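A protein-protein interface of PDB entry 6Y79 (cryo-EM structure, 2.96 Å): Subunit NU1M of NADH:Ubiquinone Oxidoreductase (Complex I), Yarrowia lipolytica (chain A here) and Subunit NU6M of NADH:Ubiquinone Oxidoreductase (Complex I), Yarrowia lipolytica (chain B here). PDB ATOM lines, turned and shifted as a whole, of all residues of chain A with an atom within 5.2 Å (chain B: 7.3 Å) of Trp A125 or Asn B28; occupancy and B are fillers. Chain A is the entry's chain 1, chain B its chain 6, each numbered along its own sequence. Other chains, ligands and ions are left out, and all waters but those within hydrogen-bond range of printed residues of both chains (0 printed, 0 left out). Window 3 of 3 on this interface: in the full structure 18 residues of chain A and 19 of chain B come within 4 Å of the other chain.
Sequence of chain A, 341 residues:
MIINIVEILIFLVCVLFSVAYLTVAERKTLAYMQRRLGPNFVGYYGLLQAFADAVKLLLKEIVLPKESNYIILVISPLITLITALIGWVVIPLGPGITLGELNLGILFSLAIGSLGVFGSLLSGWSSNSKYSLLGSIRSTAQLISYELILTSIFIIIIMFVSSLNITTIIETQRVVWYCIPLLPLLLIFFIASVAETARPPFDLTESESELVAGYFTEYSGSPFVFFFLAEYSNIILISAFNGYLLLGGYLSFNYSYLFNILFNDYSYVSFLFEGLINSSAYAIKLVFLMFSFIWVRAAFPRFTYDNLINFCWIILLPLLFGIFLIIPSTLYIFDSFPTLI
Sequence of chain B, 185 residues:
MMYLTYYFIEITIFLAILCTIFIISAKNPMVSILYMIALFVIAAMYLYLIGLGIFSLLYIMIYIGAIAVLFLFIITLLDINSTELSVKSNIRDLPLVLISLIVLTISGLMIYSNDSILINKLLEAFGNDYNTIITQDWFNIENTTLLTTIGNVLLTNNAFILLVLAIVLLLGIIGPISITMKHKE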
ATOM      1  N   ASN A  69     -16.247 -30.511   2.317  1.00  0.00           N
ATOM      2  CA  ASN A  69     -14.967 -29.985   1.894  1.00  0.00           C
ATOM      3  C   ASN A  69     -14.207 -29.711   3.180  1.00  0.00           C
ATOM      4  O   ASN A  69     -14.733 -29.027   4.073  1.00  0.00           O
ATOM      5  CB  ASN A  69     -15.129 -28.674   1.162  1.00  0.00           C
ATOM      6  CG  ASN A  69     -16.193 -28.718   0.117  1.00  0.00           C
ATOM      7  OD1 ASN A  69     -17.329 -28.318   0.386  1.00  0.00           O
ATOM      8  ND2 ASN A  69     -15.843 -29.117  -1.090  1.00  0.00           N
ATOM      9  N   LEU A 121     -22.432 -17.888   3.654  1.00  0.00           N
ATOM     10  CA  LEU A 121     -22.901 -18.617   2.476  1.00  0.00           C
ATOM     11  C   LEU A 121     -21.972 -19.760   2.101  1.00  0.00           C
ATOM     12  O   LEU A 121     -22.420 -20.901   1.923  1.00  0.00           O
ATOM     13  CB  LEU A 121     -23.026 -17.648   1.303  1.00  0.00           C
ATOM     14  CG  LEU A 121     -23.672 -18.120   0.009  1.00  0.00           C
ATOM     15  CD1 LEU A 121     -25.078 -18.618   0.271  1.00  0.00           C
ATOM     16  CD2 LEU A 121     -23.686 -16.968  -0.961  1.00  0.00           C
ATOM     17  N   LEU A 122     -20.672 -19.461   2.003  1.00  0.00           N
ATOM     18  CA  LEU A 122     -19.646 -20.451   1.695  1.00  0.00           C
ATOM     19  C   LEU A 122     -19.650 -21.595   2.697  1.00  0.00           C
ATOM     20  O   LEU A 122     -19.571 -22.765   2.308  1.00  0.00           O
ATOM     21  CB  LEU A 122     -18.290 -19.751   1.657  1.00  0.00           C
ATOM     22  CG  LEU A 122     -16.892 -20.297   1.512  1.00  0.00           C
ATOM     23  CD1 LEU A 122     -16.646 -20.498   0.072  1.00  0.00           C
ATOM     24  CD2 LEU A 122     -15.949 -19.234   2.048  1.00  0.00           C
ATOM     25  N   SER A 123     -19.839 -21.291   3.981  1.00  0.00           N
ATOM     26  CA  SER A 123     -19.803 -22.363   4.965  1.00  0.00           C
ATOM     27  C   SER A 123     -21.125 -23.108   5.053  1.00  0.00           C
ATOM     28  O   SER A 123     -21.237 -24.062   5.823  1.00  0.00           O
ATOM     29  CB  SER A 123     -19.413 -21.819   6.338  1.00  0.00           C
ATOM     30  OG  SER A 123     -20.416 -20.964   6.844  1.00  0.00           O
ATOM     31  N   GLY A 124     -22.137 -22.684   4.306  1.00  0.00           N
ATOM     32  CA  GLY A 124     -23.264 -23.562   4.080  1.00  0.00           C
ATOM     33  C   GLY A 124     -22.909 -24.703   3.157  1.00  0.00           C
ATOM     34  O   GLY A 124     -23.449 -25.809   3.289  1.00  0.00           O
ATOM     35  N   TRP A 125     -21.982 -24.456   2.222  1.00  0.00           N
ATOM     36  CA  TRP A 125     -21.539 -25.509   1.317  1.00  0.00           C
ATOM     37  C   TRP A 125     -20.652 -26.516   2.035  1.00  0.00           C
ATOM     38  O   TRP A 125     -20.461 -27.641   1.566  1.00  0.00           O
ATOM     39  CB  TRP A 125     -20.807 -24.916   0.116  1.00  0.00           C
ATOM     40  CG  TRP A 125     -20.604 -25.897  -1.020  1.00  0.00           C
ATOM     41  CD1 TRP A 125     -19.516 -26.706  -1.216  1.00  0.00           C
ATOM     42  CD2 TRP A 125     -21.499 -26.162  -2.114  1.00  0.00           C
ATOM     43  NE1 TRP A 125     -19.686 -27.466  -2.348  1.00  0.00           N
ATOM     44  CE2 TRP A 125     -20.891 -27.149  -2.921  1.00  0.00           C
ATOM     45  CE3 TRP A 125     -22.751 -25.665  -2.489  1.00  0.00           C
ATOM     46  CZ2 TRP A 125     -21.495 -27.646  -4.082  1.00  0.00           C
ATOM     47  CZ3 TRP A 125     -23.349 -26.165  -3.638  1.00  0.00           C
ATOM     48  CH2 TRP A 125     -22.719 -27.141  -4.420  1.00  0.00           C
ATOM     49  N   SER A 126     -20.094 -26.127   3.162  1.00  0.00           N
ATOM     50  CA  SER A 126     -19.547 -27.094   4.088  1.00  0.00           C
ATOM     51  C   SER A 126     -20.655 -27.975   4.650  1.00  0.00           C
ATOM     52  O   SER A 126     -21.727 -27.483   5.021  1.00  0.00           O
ATOM     53  CB  SER A 126     -18.884 -26.374   5.224  1.00  0.00           C
ATOM     54  OG  SER A 126     -17.887 -25.468   4.802  1.00  0.00           O
ATOM     55  N   SER A 127     -20.361 -29.277   4.741  1.00  0.00           N
ATOM     56  CA  SER A 127     -21.258 -30.330   5.243  1.00  0.00           C
ATOM     57  C   SER A 127     -22.585 -30.348   4.483  1.00  0.00           C
ATOM     58  O   SER A 127     -23.654 -30.131   5.064  1.00  0.00           O
ATOM     59  CB  SER A 127     -21.495 -30.213   6.754  1.00  0.00           C
ATOM     60  OG  SER A 127     -22.284 -29.083   7.075  1.00  0.00           O
ATOM     61  N   ASN A 128     -22.504 -30.638   3.171  1.00  0.00           N
ATOM     62  CA  ASN A 128     -23.632 -30.455   2.269  1.00  0.00           C
ATOM     63  C   ASN A 128     -24.787 -31.386   2.593  1.00  0.00           C
ATOM     64  O   ASN A 128     -24.896 -32.508   2.090  1.00  0.00           O
ATOM     65  CB  ASN A 128     -23.167 -30.664   0.832  1.00  0.00           C
ATOM     66  CG  ASN A 128     -22.915 -29.352   0.104  1.00  0.00           C
ATOM     67  OD1 ASN A 128     -23.167 -28.280   0.653  1.00  0.00           O
ATOM     68  ND2 ASN A 128     -22.412 -29.430  -1.126  1.00  0.00           N
ATOM     69  N   SER A 132     -28.625 -28.048   5.639  1.00  0.00           N
ATOM     70  CA  SER A 132     -27.415 -27.273   5.864  1.00  0.00           C
ATOM     71  C   SER A 132     -27.173 -26.267   4.759  1.00  0.00           C
ATOM     72  O   SER A 132     -26.160 -25.561   4.788  1.00  0.00           O
ATOM     73  CB  SER A 132     -26.193 -28.172   5.969  1.00  0.00           C
ATOM     74  OG  SER A 132     -25.756 -28.549   4.687  1.00  0.00           O
ATOM     75  N   LEU A 133     -28.058 -26.215   3.769  1.00  0.00           N
ATOM     76  CA  LEU A 133     -27.945 -25.284   2.659  1.00  0.00           C
ATOM     77  C   LEU A 133     -28.962 -24.163   2.740  1.00  0.00           C
ATOM     78  O   LEU A 133     -28.587 -22.991   2.645  1.00  0.00           O
ATOM     79  CB  LEU A 133     -28.104 -26.021   1.324  1.00  0.00           C
ATOM     80  CG  LEU A 133     -26.994 -26.987   0.930  1.00  0.00           C
ATOM     81  CD1 LEU A 133     -27.338 -27.701  -0.363  1.00  0.00           C
ATOM     82  CD2 LEU A 133     -25.706 -26.230   0.800  1.00  0.00           C
ATOM     83  N   ILE B  23      -9.550 -21.363 -12.957  1.00  0.00           N
ATOM     84  CA  ILE B  23     -10.992 -21.183 -13.144  1.00  0.00           C
ATOM     85  C   ILE B  23     -11.542 -22.242 -14.089  1.00  0.00           C
ATOM     86  O   ILE B  23     -12.522 -22.929 -13.776  1.00  0.00           O
ATOM     87  CB  ILE B  23     -11.310 -19.765 -13.662  1.00  0.00           C
ATOM     88  CG1 ILE B  23     -11.216 -18.729 -12.557  1.00  0.00           C
ATOM     89  CG2 ILE B  23     -12.708 -19.687 -14.241  1.00  0.00           C
ATOM     90  CD1 ILE B  23     -11.099 -17.339 -13.064  1.00  0.00           C
ATOM     91  N   SER B  25     -10.482 -25.132 -15.046  1.00  0.00           N
ATOM     92  CA  SER B  25     -10.210 -26.540 -14.745  1.00  0.00           C
ATOM     93  C   SER B  25     -10.367 -26.743 -13.239  1.00  0.00           C
ATOM     94  O   SER B  25      -9.404 -26.555 -12.494  1.00  0.00           O
ATOM     95  CB  SER B  25      -8.824 -26.935 -15.214  1.00  0.00           C
ATOM     96  OG  SER B  25      -7.821 -26.256 -14.480  1.00  0.00           O
ATOM     97  N   ALA B  26     -11.563 -27.136 -12.781  1.00  0.00           N
ATOM     98  CA  ALA B  26     -11.807 -27.205 -11.341  1.00  0.00           C
ATOM     99  C   ALA B  26     -12.868 -28.245 -11.025  1.00  0.00           C
ATOM    100  O   ALA B  26     -13.841 -28.359 -11.770  1.00  0.00           O
ATOM    101  CB  ALA B  26     -12.236 -25.841 -10.799  1.00  0.00           C
ATOM    102  N   LYS B  27     -12.685 -28.945  -9.895  1.00  0.00           N
ATOM    103  CA  LYS B  27     -13.336 -30.223  -9.608  1.00  0.00           C
ATOM    104  C   LYS B  27     -14.856 -30.141  -9.644  1.00  0.00           C
ATOM    105  O   LYS B  27     -15.484 -30.687 -10.553  1.00  0.00           O
ATOM    106  CB  LYS B  27     -12.809 -30.729  -8.281  1.00  0.00           C
ATOM    107  CG  LYS B  27     -12.629 -29.611  -7.252  1.00  0.00           C
ATOM    108  CD  LYS B  27     -12.310 -30.032  -5.817  1.00  0.00           C
ATOM    109  CE  LYS B  27     -10.856 -30.147  -5.589  1.00  0.00           C
ATOM    110  NZ  LYS B  27     -10.401 -28.765  -5.838  1.00  0.00           N
ATOM    111  N   ASN B  28     -15.430 -29.357  -8.786  1.00  0.00           N
ATOM    112  CA  ASN B  28     -16.537 -28.676  -8.136  1.00  0.00           C
ATOM    113  C   ASN B  28     -16.724 -27.301  -8.764  1.00  0.00           C
ATOM    114  O   ASN B  28     -15.751 -26.552  -8.913  1.00  0.00           O
ATOM    115  CB  ASN B  28     -16.297 -28.524  -6.618  1.00  0.00           C
ATOM    116  CG  ASN B  28     -17.571 -28.454  -5.848  1.00  0.00           C
ATOM    117  OD1 ASN B  28     -18.559 -29.135  -6.205  1.00  0.00           O
ATOM    118  ND2 ASN B  28     -17.563 -27.736  -4.766  1.00  0.00           N
ATOM    119  N   PRO B  29     -17.981 -27.040  -9.132  1.00  0.00           N
ATOM    120  CA  PRO B  29     -18.345 -25.753  -9.742  1.00  0.00           C
ATOM    121  C   PRO B  29     -18.038 -24.518  -8.876  1.00  0.00           C
ATOM    122  O   PRO B  29     -17.653 -23.462  -9.403  1.00  0.00           O
ATOM    123  CB  PRO B  29     -19.841 -25.951  -9.975  1.00  0.00           C
ATOM    124  CG  PRO B  29     -20.244 -27.208  -9.252  1.00  0.00           C
ATOM    125  CD  PRO B  29     -19.055 -28.034  -9.269  1.00  0.00           C
ATOM    126  N   MET B  30     -18.141 -24.626  -7.544  1.00  0.00           N
ATOM    127  CA  MET B  30     -17.895 -23.467  -6.684  1.00  0.00           C
ATOM    128  C   MET B  30     -16.415 -23.322  -6.328  1.00  0.00           C
ATOM    129  O   MET B  30     -15.991 -22.254  -5.901  1.00  0.00           O
ATOM    130  CB  MET B  30     -18.765 -23.506  -5.415  1.00  0.00           C
ATOM    131  CG  MET B  30     -18.585 -24.612  -4.376  1.00  0.00           C
ATOM    132  SD  MET B  30     -17.331 -24.290  -3.133  1.00  0.00           S
ATOM    133  CE  MET B  30     -17.929 -22.728  -2.525  1.00  0.00           C
ATOM    134  N   VAL B  31     -15.600 -24.360  -6.526  1.00  0.00           N
ATOM    135  CA  VAL B  31     -14.152 -24.157  -6.479  1.00  0.00           C
ATOM    136  C   VAL B  31     -13.726 -23.234  -7.612  1.00  0.00           C
ATOM    137  O   VAL B  31     -12.983 -22.260  -7.407  1.00  0.00           O
ATOM    138  CB  VAL B  31     -13.457 -25.529  -6.522  1.00  0.00           C
ATOM    139  CG1 VAL B  31     -11.991 -25.393  -6.795  1.00  0.00           C
ATOM    140  CG2 VAL B  31     -13.670 -26.272  -5.189  1.00  0.00           C
ATOM    141  N   SER B  32     -14.302 -23.464  -8.792  1.00  0.00           N
ATOM    142  CA  SER B  32     -14.167 -22.568  -9.932  1.00  0.00           C
ATOM    143  C   SER B  32     -14.681 -21.154  -9.614  1.00  0.00           C
ATOM    144  O   SER B  32     -14.022 -20.158  -9.955  1.00  0.00           O
ATOM    145  CB  SER B  32     -14.881 -23.229 -11.116  1.00  0.00           C
ATOM    146  OG  SER B  32     -15.140 -22.381 -12.174  1.00  0.00           O
ATOM    147  N   ILE B  33     -15.805 -21.023  -8.905  1.00  0.00           N
ATOM    148  CA  ILE B  33     -16.271 -19.659  -8.623  1.00  0.00           C
ATOM    149  C   ILE B  33     -15.401 -18.925  -7.588  1.00  0.00           C
ATOM    150  O   ILE B  33     -15.272 -17.689  -7.639  1.00  0.00           O
ATOM    151  CB  ILE B  33     -17.748 -19.670  -8.224  1.00  0.00           C
ATOM    152  CG1 ILE B  33     -18.304 -18.325  -8.549  1.00  0.00           C
ATOM    153  CG2 ILE B  33     -17.963 -19.848  -6.756  1.00  0.00           C
ATOM    154  CD1 ILE B  33     -19.615 -18.429  -8.604  1.00  0.00           C
ATOM    155  N   TYR B  35     -12.159 -19.296  -7.399  1.00  0.00           N
ATOM    156  CA  TYR B  35     -11.060 -18.803  -8.220  1.00  0.00           C
ATOM    157  C   TYR B  35     -11.449 -17.543  -8.990  1.00  0.00           C
ATOM    158  O   TYR B  35     -10.602 -16.666  -9.196  1.00  0.00           O
ATOM    159  CB  TYR B  35     -10.577 -19.878  -9.184  1.00  0.00           C
ATOM    160  CG  TYR B  35      -9.838 -21.016  -8.544  1.00  0.00           C
ATOM    161  CD1 TYR B  35      -8.753 -20.796  -7.711  1.00  0.00           C
ATOM    162  CD2 TYR B  35     -10.201 -22.319  -8.812  1.00  0.00           C
ATOM    163  CE1 TYR B  35      -8.075 -21.858  -7.140  1.00  0.00           C
ATOM    164  CE2 TYR B  35      -9.529 -23.371  -8.262  1.00  0.00           C
ATOM    165  CZ  TYR B  35      -8.477 -23.142  -7.421  1.00  0.00           C
ATOM    166  OH  TYR B  35      -7.828 -24.223  -6.877  1.00  0.00           O
ATOM    167  N   LEU B  72     -22.805 -17.469  -6.180  1.00  0.00           N
ATOM    168  CA  LEU B  72     -22.707 -18.525  -5.166  1.00  0.00           C
ATOM    169  C   LEU B  72     -24.079 -18.915  -4.638  1.00  0.00           C
ATOM    170  O   LEU B  72     -24.357 -20.101  -4.400  1.00  0.00           O
ATOM    171  CB  LEU B  72     -21.838 -18.066  -3.994  1.00  0.00           C
ATOM    172  CG  LEU B  72     -20.351 -18.355  -3.801  1.00  0.00           C
ATOM    173  CD1 LEU B  72     -19.516 -17.429  -4.595  1.00  0.00           C
ATOM    174  CD2 LEU B  72     -20.009 -18.163  -2.362  1.00  0.00           C
ATOM    175  N   ILE B  74     -26.754 -18.832  -6.357  1.00  0.00           N
ATOM    176  CA  ILE B  74     -27.383 -19.663  -7.385  1.00  0.00           C
ATOM    177  C   ILE B  74     -26.881 -21.100  -7.296  1.00  0.00           C
ATOM    178  O   ILE B  74     -27.670 -22.050  -7.355  1.00  0.00           O
ATOM    179  CB  ILE B  74     -27.140 -19.068  -8.787  1.00  0.00           C
ATOM    180  CG1 ILE B  74     -27.938 -17.786  -8.979  1.00  0.00           C
ATOM    181  CG2 ILE B  74     -27.529 -20.043  -9.885  1.00  0.00           C
ATOM    182  CD1 ILE B  74     -29.404 -17.958  -8.971  1.00  0.00           C
ATOM    183  N   ILE B  75     -25.565 -21.279  -7.145  1.00  0.00           N
ATOM    184  CA  ILE B  75     -24.979 -22.626  -7.143  1.00  0.00           C
ATOM    185  C   ILE B  75     -25.441 -23.446  -5.947  1.00  0.00           C
ATOM    186  O   ILE B  75     -25.585 -24.673  -6.047  1.00  0.00           O
ATOM    187  CB  ILE B  75     -23.448 -22.523  -7.183  1.00  0.00           C
ATOM    188  CG1 ILE B  75     -23.032 -21.816  -8.440  1.00  0.00           C
ATOM    189  CG2 ILE B  75     -22.757 -23.878  -7.210  1.00  0.00           C
ATOM    190  CD1 ILE B  75     -21.702 -21.310  -8.293  1.00  0.00           C
ATOM    191  N   THR B  76     -25.709 -22.792  -4.817  1.00  0.00           N
ATOM    192  CA  THR B  76     -26.175 -23.505  -3.633  1.00  0.00           C
ATOM    193  C   THR B  76     -27.498 -24.246  -3.826  1.00  0.00           C
ATOM    194  O   THR B  76     -27.532 -25.473  -3.696  1.00  0.00           O
ATOM    195  CB  THR B  76     -26.295 -22.544  -2.458  1.00  0.00           C
ATOM    196  OG1 THR B  76     -25.051 -21.867  -2.273  1.00  0.00           O
ATOM    197  CG2 THR B  76     -26.626 -23.299  -1.213  1.00  0.00           C
ATOM    198  N   LEU B  77     -28.580 -23.549  -4.164  1.00  0.00           N
ATOM    199  CA  LEU B  77     -29.890 -24.185  -4.177  1.00  0.00           C
ATOM    200  C   LEU B  77     -30.367 -24.595  -5.567  1.00  0.00           C
ATOM    201  O   LEU B  77     -31.570 -24.773  -5.769  1.00  0.00           O
ATOM    202  CB  LEU B  77     -30.922 -23.295  -3.474  1.00  0.00           C
ATOM    203  CG  LEU B  77     -31.151 -21.796  -3.692  1.00  0.00           C
ATOM    204  CD1 LEU B  77     -31.997 -21.518  -4.871  1.00  0.00           C
ATOM    205  CD2 LEU B  77     -31.901 -21.279  -2.518  1.00  0.00           C
ATOM    206  N   LEU B  78     -29.457 -24.805  -6.511  1.00  0.00           N
ATOM    207  CA  LEU B  78     -29.805 -25.368  -7.808  1.00  0.00           C
ATOM    208  C   LEU B  78     -28.864 -26.522  -8.120  1.00  0.00           C
ATOM    209  O   LEU B  78     -27.726 -26.560  -7.652  1.00  0.00           O
ATOM    210  CB  LEU B  78     -29.746 -24.324  -8.930  1.00  0.00           C
ATOM    211  CG  LEU B  78     -30.950 -23.392  -9.088  1.00  0.00           C
ATOM    212  CD1 LEU B  78     -30.838 -22.196  -8.223  1.00  0.00           C
ATOM    213  CD2 LEU B  78     -31.064 -22.936 -10.485  1.00  0.00           C
ATOM    214  N   SER B  82     -21.735 -31.745 -13.634  1.00  0.00           N
ATOM    215  CA  SER B  82     -20.429 -31.334 -14.124  1.00  0.00           C
ATOM    216  C   SER B  82     -19.595 -32.567 -14.431  1.00  0.00           C
ATOM    217  O   SER B  82     -19.480 -33.470 -13.599  1.00  0.00           O
ATOM    218  CB  SER B  82     -19.707 -30.447 -13.100  1.00  0.00           C
ATOM    219  OG  SER B  82     -18.475 -29.951 -13.599  1.00  0.00           O
ATOM    220  N   THR B  83     -19.016 -32.599 -15.623  1.00  0.00           N
ATOM    221  CA  THR B  83     -17.934 -33.522 -15.918  1.00  0.00           C
ATOM    222  C   THR B  83     -16.631 -32.853 -15.512  1.00  0.00           C
ATOM    223  O   THR B  83     -16.531 -31.627 -15.510  1.00  0.00           O
ATOM    224  CB  THR B  83     -17.899 -33.896 -17.404  1.00  0.00           C
ATOM    225  OG1 THR B  83     -17.197 -32.891 -18.147  1.00  0.00           O
ATOM    226  CG2 THR B  83     -19.302 -34.018 -17.959  1.00  0.00           C
ATOM    227  N   GLU B  84     -15.645 -33.643 -15.113  1.00  0.00           N
ATOM    228  CA  GLU B  84     -14.379 -32.985 -14.855  1.00  0.00           C
ATOM    229  C   GLU B  84     -13.472 -33.125 -16.075  1.00  0.00           C
ATOM    230  O   GLU B  84     -13.754 -33.884 -17.004  1.00  0.00           O
ATOM    231  CB  GLU B  84     -13.709 -33.526 -13.587  1.00  0.00           C
ATOM    232  CG  GLU B  84     -12.913 -32.432 -12.871  1.00  0.00           C
ATOM    233  CD  GLU B  84     -12.232 -32.879 -11.624  1.00  0.00           C
ATOM    234  OE1 GLU B  84     -11.184 -32.274 -11.291  1.00  0.00           O
ATOM    235  OE2 GLU B  84     -12.742 -33.791 -10.936  1.00  0.00           O
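Among the printed residues, pairs that only touch across the chains: Leu A121 with Leu B72, Leu A122 with Met B30, Trp A125 with Met B30, Trp A125 with Ile B75, Trp A125 with Thr B76 and Leu A133 with Thr B76.
The side-chain amide oxygen of Asn A69 sits close to the backbone carbonyl oxygen of Trp A125, at 3.4 Å. The side-chain amide oxygen (OD1) of Asn A128 lies close to the backbone carbonyl oxygen (O) of Trp A125, 2.9 Å away. The side-chain hydroxyl of Thr B76 lies within hydrogen-bond range of the backbone carbonyl oxygen of Leu B72, at 2.9 Å.
Of the 20 printed residues of chain B, 5 touch a printed residue of chain A. Printed residues of chain B that touch a printed residue of chain A: Asn B28, Met B30, Leu B72, Ile B75 and Thr B76. Hydrophobic or aromatic side chains of chain B within 4 Å of the printed part of chain A: Met B30 and Leu B72. Along chain B the printed residues that touch a printed residue of chain A span positions 28 to 76. Of the 11 printed residues of chain A, 4 touch a printed residue of chain B. Among the printed residues, no Asp or Glu carboxylate lies within 4 Å of a Lys or Arg side-chain nitrogen of the other chain.
ND2 of Asn B28 sits close to NE1 of Trp A125, 3.2 Å away.
Of the printed residues of chain A, Asn B28 touches Trp A125 (3.2 Å). Of the printed residues of chain B, Leu A121 touches Leu B72. Printed residues of chain A within 4 Å of Leu B72: Leu A121. Of the printed residues of chain A, Thr B76 touches Trp A125 and Leu A133. Of the printed residues of chain A, Met B30 touches Leu A122 (3.7 Å) and Trp A125 (3.7 Å). Ser B32 touches none of the printed residues of chain A. Ser B25 touches none of the printed residues of chain A. The nearest residue of chain B that does not touch Trp A125 is Pro B29 (5.3 Å). The nearest residue of chain A that does not touch Asn B28 is Asn A69 (4.3 Å). The nearest printed residue of chain B that does not touch Leu A122 is Leu B72 (4.6 Å).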
